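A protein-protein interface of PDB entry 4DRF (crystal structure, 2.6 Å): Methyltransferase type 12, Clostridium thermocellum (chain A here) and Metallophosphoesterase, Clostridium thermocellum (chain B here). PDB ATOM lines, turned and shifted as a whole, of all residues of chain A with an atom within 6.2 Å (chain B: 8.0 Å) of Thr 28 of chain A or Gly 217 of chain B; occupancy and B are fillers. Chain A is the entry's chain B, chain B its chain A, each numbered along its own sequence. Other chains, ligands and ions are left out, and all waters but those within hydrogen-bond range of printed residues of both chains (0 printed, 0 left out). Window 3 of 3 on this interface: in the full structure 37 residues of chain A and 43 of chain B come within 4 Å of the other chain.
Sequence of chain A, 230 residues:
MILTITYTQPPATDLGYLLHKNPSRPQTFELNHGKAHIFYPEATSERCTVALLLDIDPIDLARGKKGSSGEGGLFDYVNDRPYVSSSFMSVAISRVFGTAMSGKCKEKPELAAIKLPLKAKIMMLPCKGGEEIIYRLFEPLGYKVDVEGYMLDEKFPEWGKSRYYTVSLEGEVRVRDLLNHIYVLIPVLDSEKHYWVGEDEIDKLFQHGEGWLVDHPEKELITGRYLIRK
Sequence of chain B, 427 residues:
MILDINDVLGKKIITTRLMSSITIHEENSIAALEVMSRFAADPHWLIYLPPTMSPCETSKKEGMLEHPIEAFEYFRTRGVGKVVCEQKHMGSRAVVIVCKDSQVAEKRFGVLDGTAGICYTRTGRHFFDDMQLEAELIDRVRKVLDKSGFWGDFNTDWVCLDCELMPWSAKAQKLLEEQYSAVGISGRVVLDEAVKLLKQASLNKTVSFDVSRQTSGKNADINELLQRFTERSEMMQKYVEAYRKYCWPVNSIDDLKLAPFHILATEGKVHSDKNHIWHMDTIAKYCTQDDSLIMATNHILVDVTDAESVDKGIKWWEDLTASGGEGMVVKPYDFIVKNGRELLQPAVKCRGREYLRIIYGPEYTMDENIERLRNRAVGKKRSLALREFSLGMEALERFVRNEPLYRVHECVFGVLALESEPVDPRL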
ATOM      1  N   LYS A  21      15.118  34.105  14.112  1.00  0.00           N
ATOM      2  CA  LYS A  21      15.937  33.415  15.078  1.00  0.00           C
ATOM      3  C   LYS A  21      17.255  34.133  14.931  1.00  0.00           C
ATOM      4  O   LYS A  21      17.876  34.127  13.860  1.00  0.00           O
ATOM      5  CB  LYS A  21      16.000  31.915  14.781  1.00  0.00           C
ATOM      6  CG  LYS A  21      14.620  31.234  15.002  1.00  0.00           C
ATOM      7  CD  LYS A  21      14.190  31.335  16.460  1.00  0.00           C
ATOM      8  CE  LYS A  21      12.805  30.774  16.695  1.00  0.00           C
ATOM      9  NZ  LYS A  21      11.834  31.283  15.691  1.00  0.00           N
ATOM     10  N   PRO A  26      21.074  30.028  19.496  1.00  0.00           N
ATOM     11  CA  PRO A  26      20.542  28.679  19.266  1.00  0.00           C
ATOM     12  C   PRO A  26      19.403  28.356  20.222  1.00  0.00           C
ATOM     13  O   PRO A  26      19.416  28.731  21.398  1.00  0.00           O
ATOM     14  CB  PRO A  26      21.742  27.759  19.525  1.00  0.00           C
ATOM     15  CG  PRO A  26      22.793  28.624  20.131  1.00  0.00           C
ATOM     16  CD  PRO A  26      22.526  30.019  19.718  1.00  0.00           C
ATOM     17  N   GLN A  27      18.397  27.680  19.691  1.00  0.00           N
ATOM     18  CA  GLN A  27      17.214  27.384  20.467  1.00  0.00           C
ATOM     19  C   GLN A  27      16.736  25.949  20.341  1.00  0.00           C
ATOM     20  O   GLN A  27      17.018  25.262  19.360  1.00  0.00           O
ATOM     21  CB  GLN A  27      16.094  28.347  20.102  1.00  0.00           C
ATOM     22  CG  GLN A  27      16.418  29.771  20.475  1.00  0.00           C
ATOM     23  CD  GLN A  27      15.187  30.611  20.633  1.00  0.00           C
ATOM     24  OE1 GLN A  27      14.408  30.791  19.687  1.00  0.00           O
ATOM     25  NE2 GLN A  27      14.987  31.130  21.844  1.00  0.00           N
ATOM     26  N   THR A  28      16.010  25.516  21.367  1.00  0.00           N
ATOM     27  CA  THR A  28      15.401  24.202  21.399  1.00  0.00           C
ATOM     28  C   THR A  28      13.897  24.347  21.631  1.00  0.00           C
ATOM     29  O   THR A  28      13.466  25.094  22.504  1.00  0.00           O
ATOM     30  CB  THR A  28      16.051  23.301  22.500  1.00  0.00           C
ATOM     31  OG1 THR A  28      17.382  22.921  22.110  1.00  0.00           O
ATOM     32  CG2 THR A  28      15.237  22.040  22.721  1.00  0.00           C
ATOM     33  N   PHE A  29      13.115  23.652  20.816  1.00  0.00           N
ATOM     34  CA  PHE A  29      11.666  23.612  20.930  1.00  0.00           C
ATOM     35  C   PHE A  29      11.236  22.175  21.225  1.00  0.00           C
ATOM     36  O   PHE A  29      11.831  21.250  20.699  1.00  0.00           O
ATOM     37  CB  PHE A  29      11.022  24.068  19.618  1.00  0.00           C
ATOM     38  CG  PHE A  29      11.128  25.531  19.374  1.00  0.00           C
ATOM     39  CD1 PHE A  29      12.360  26.120  19.184  1.00  0.00           C
ATOM     40  CD2 PHE A  29       9.994  26.321  19.334  1.00  0.00           C
ATOM     41  CE1 PHE A  29      12.463  27.475  18.966  1.00  0.00           C
ATOM     42  CE2 PHE A  29      10.089  27.679  19.114  1.00  0.00           C
ATOM     43  CZ  PHE A  29      11.326  28.256  18.928  1.00  0.00           C
ATOM     44  N   GLU A  30      10.201  21.982  22.043  1.00  0.00           N
ATOM     45  CA  GLU A  30       9.747  20.633  22.398  1.00  0.00           C
ATOM     46  C   GLU A  30       8.511  20.173  21.634  1.00  0.00           C
ATOM     47  O   GLU A  30       7.481  20.833  21.659  1.00  0.00           O
ATOM     48  CB  GLU A  30       9.541  20.507  23.910  1.00  0.00           C
ATOM     49  CG  GLU A  30       8.964  21.752  24.575  1.00  0.00           C
ATOM     50  CD  GLU A  30       8.949  21.663  26.100  1.00  0.00           C
ATOM     51  OE1 GLU A  30       9.597  20.753  26.657  1.00  0.00           O
ATOM     52  OE2 GLU A  30       8.286  22.507  26.742  1.00  0.00           O
ATOM     53  N   LYS A  35      12.052  16.645  20.366  1.00  0.00           N
ATOM     54  CA  LYS A  35      12.281  18.080  20.367  1.00  0.00           C
ATOM     55  C   LYS A  35      13.124  18.533  19.169  1.00  0.00           C
ATOM     56  O   LYS A  35      13.643  17.725  18.414  1.00  0.00           O
ATOM     57  CB  LYS A  35      12.827  18.566  21.714  1.00  0.00           C
ATOM     58  CG  LYS A  35      14.237  18.212  22.002  1.00  0.00           C
ATOM     59  CD  LYS A  35      14.525  18.381  23.488  1.00  0.00           C
ATOM     60  CE  LYS A  35      15.877  17.777  23.870  1.00  0.00           C
ATOM     61  NZ  LYS A  35      15.918  16.294  23.694  1.00  0.00           N
ATOM     62  N   ALA A  36      13.192  19.836  18.954  1.00  0.00           N
ATOM     63  CA  ALA A  36      13.789  20.372  17.733  1.00  0.00           C
ATOM     64  C   ALA A  36      14.757  21.510  18.074  1.00  0.00           C
ATOM     65  O   ALA A  36      14.478  22.329  18.940  1.00  0.00           O
ATOM     66  CB  ALA A  36      12.694  20.836  16.782  1.00  0.00           C
ATOM     67  N   HIS A  37      15.912  21.521  17.424  1.00  0.00           N
ATOM     68  CA  HIS A  37      16.916  22.541  17.657  1.00  0.00           C
ATOM     69  C   HIS A  37      17.075  23.384  16.404  1.00  0.00           C
ATOM     70  O   HIS A  37      17.100  22.854  15.287  1.00  0.00           O
ATOM     71  CB  HIS A  37      18.246  21.900  17.982  1.00  0.00           C
ATOM     72  CG  HIS A  37      18.142  20.777  18.958  1.00  0.00           C
ATOM     73  ND1 HIS A  37      17.828  20.973  20.289  1.00  0.00           N
ATOM     74  CD2 HIS A  37      18.292  19.440  18.803  1.00  0.00           C
ATOM     75  CE1 HIS A  37      17.792  19.809  20.905  1.00  0.00           C
ATOM     76  NE2 HIS A  37      18.068  18.862  20.026  1.00  0.00           N
ATOM     77  N   ILE A  38      17.168  24.697  16.597  1.00  0.00           N
ATOM     78  CA  ILE A  38      17.423  25.627  15.507  1.00  0.00           C
ATOM     79  C   ILE A  38      18.664  26.430  15.855  1.00  0.00           C
ATOM     80  O   ILE A  38      18.820  26.928  16.974  1.00  0.00           O
ATOM     81  CB  ILE A  38      16.186  26.521  15.232  1.00  0.00           C
ATOM     82  CG1 ILE A  38      16.280  27.202  13.867  1.00  0.00           C
ATOM     83  CG2 ILE A  38      15.958  27.534  16.357  1.00  0.00           C
ATOM     84  CD1 ILE A  38      16.698  28.606  13.935  1.00  0.00           C
ATOM     85  N   GLY B 217      11.108  29.055  21.964  1.00  0.00           N
ATOM     86  CA  GLY B 217      11.313  27.936  22.858  1.00  0.00           C
ATOM     87  C   GLY B 217      12.272  28.331  23.957  1.00  0.00           C
ATOM     88  O   GLY B 217      12.056  29.319  24.663  1.00  0.00           O
ATOM     89  N   LYS B 218      13.337  27.553  24.118  1.00  0.00           N
ATOM     90  CA  LYS B 218      14.326  27.839  25.161  1.00  0.00           C
ATOM     91  C   LYS B 218      15.746  27.865  24.624  1.00  0.00           C
ATOM     92  O   LYS B 218      16.009  27.404  23.519  1.00  0.00           O
ATOM     93  CB  LYS B 218      14.202  26.843  26.319  1.00  0.00           C
ATOM     94  CG  LYS B 218      14.240  25.386  25.909  1.00  0.00           C
ATOM     95  CD  LYS B 218      14.464  24.503  27.143  1.00  0.00           C
ATOM     96  CE  LYS B 218      14.736  23.053  26.746  1.00  0.00           C
ATOM     97  NZ  LYS B 218      13.499  22.342  26.332  1.00  0.00           N
ATOM     98  N   ASN B 219      16.658  28.412  25.415  1.00  0.00           N
ATOM     99  CA  ASN B 219      18.046  28.512  25.007  1.00  0.00           C
ATOM    100  C   ASN B 219      18.794  27.203  24.995  1.00  0.00           C
ATOM    101  O   ASN B 219      18.784  26.453  25.969  1.00  0.00           O
ATOM    102  CB  ASN B 219      18.803  29.514  25.893  1.00  0.00           C
ATOM    103  CG  ASN B 219      18.382  30.949  25.642  1.00  0.00           C
ATOM    104  OD1 ASN B 219      18.364  31.429  24.605  1.00  0.00           O
ATOM    105  ND2 ASN B 219      18.072  31.570  26.597  1.00  0.00           N
ATOM    106  N   ALA B 220      19.482  26.965  23.889  1.00  0.00           N
ATOM    107  CA  ALA B 220      20.333  25.802  23.772  1.00  0.00           C
ATOM    108  C   ALA B 220      21.782  26.234  23.822  1.00  0.00           C
ATOM    109  O   ALA B 220      22.115  27.357  23.466  1.00  0.00           O
ATOM    110  CB  ALA B 220      20.028  25.037  22.500  1.00  0.00           C
ATOM    111  N   ASP B 221      22.638  25.324  24.262  1.00  0.00           N
ATOM    112  CA  ASP B 221      24.078  25.516  24.199  1.00  0.00           C
ATOM    113  C   ASP B 221      24.614  24.684  23.041  1.00  0.00           C
ATOM    114  O   ASP B 221      24.339  23.487  22.951  1.00  0.00           O
ATOM    115  CB  ASP B 221      24.739  25.072  25.507  1.00  0.00           C
ATOM    116  CG  ASP B 221      26.259  25.000  25.403  1.00  0.00           C
ATOM    117  OD1 ASP B 221      26.773  23.958  24.956  1.00  0.00           O
ATOM    118  OD2 ASP B 221      26.940  25.987  25.751  1.00  0.00           O
ATOM    119  N   LEU B 225      24.972  20.425  22.722  1.00  0.00           N
ATOM    120  CA  LEU B 225      24.380  19.846  21.520  1.00  0.00           C
ATOM    121  C   LEU B 225      25.385  19.038  20.717  1.00  0.00           C
ATOM    122  O   LEU B 225      25.128  17.883  20.377  1.00  0.00           O
ATOM    123  CB  LEU B 225      23.738  20.927  20.633  1.00  0.00           C
ATOM    124  CG  LEU B 225      22.325  21.438  20.976  1.00  0.00           C
ATOM    125  CD1 LEU B 225      21.912  22.604  20.116  1.00  0.00           C
ATOM    126  CD2 LEU B 225      21.325  20.325  20.805  1.00  0.00           C
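The backbone NH (N) of Ala 220 of chain B is in hydrogen-bond range of the backbone carbonyl oxygen (O) of Pro 26 of chain A (3.1 Å). O of Lys 218 of chain B sits at hydrogen-bond distance from N of Thr 28 of chain A, at 2.9 Å.
The backbone carbonyl oxygen (O) of Gln 27 of chain A lies within hydrogen-bond range of the backbone NH (N) of Ile 38 of chain A (2.8 Å). The backbone carbonyl oxygen of Phe 29 of chain A is in hydrogen-bond range of the backbone NH of Ala 36 of chain A (2.6 Å). A ring nitrogen (ND1) of His 37 of chain A sits at hydrogen-bond distance from the side-chain hydroxyl of Thr 28 of chain A.
Asn 219 of chain B touches Pro 26 of chain A. Gln 27 of chain A touches Lys 218 of chain B (CA to O, 3.3 Å). Thr 28 of chain A touches Gly 217 of chain B (O to CA, 3.6 Å). Thr 28 of chain A touches Ala 220 of chain B (OG1 to CB, 3.4 Å). Gly 217 of chain B touches Phe 29 of chain A. CE1 of His 37 of chain A touches CD2 of Leu 225 of chain B, 3.6 Å away.
Printed residues of chain B within 4 Å of Pro 26 of chain A: Asn 219 (3.9 Å) and Ala 220 (3.1 Å). Thr 28 of chain A touches just these residues of chain B: Gly 217 (3.6 Å), Lys 218 (2.9 Å) and Ala 220 (3.4 Å). Of the printed residues of chain B, Phe 29 of chain A touches Gly 217 (3.1 Å). Glu 30 of chain A touches none of the printed residues of chain B. Printed residues of chain B within 4 Å of His 37 of chain A: Leu 225 (3.6 Å). Of the printed residues of chain A, Gly 217 of chain B touches Thr 28 (3.6 Å) and Phe 29 (3.1 Å). Of the printed residues of chain A, Leu 225 of chain B touches His 37. The nearest printed residue of chain B that does not touch Thr 28 of chain A is Asn 219 of chain B (4.9 Å). The nearest printed residue of chain B that does not touch Pro 26 of chain A is Lys 218 of chain B (4.2 Å).
Of the 6 printed residues of chain B, 5 touch a printed residue of chain A. Along chain B the printed residues that touch a printed residue of chain A span positions 217 to 225. Of the 10 printed residues of chain A, 5 touch a printed residue of chain B. Hydrophobic or aromatic side chains of chain A that line the printed part of chain B: Pro 26, Phe 29 and His 37. Among the printed residues, no Asp or Glu carboxylate lies within 4 Å of a Lys or Arg side-chain nitrogen of the other chain.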
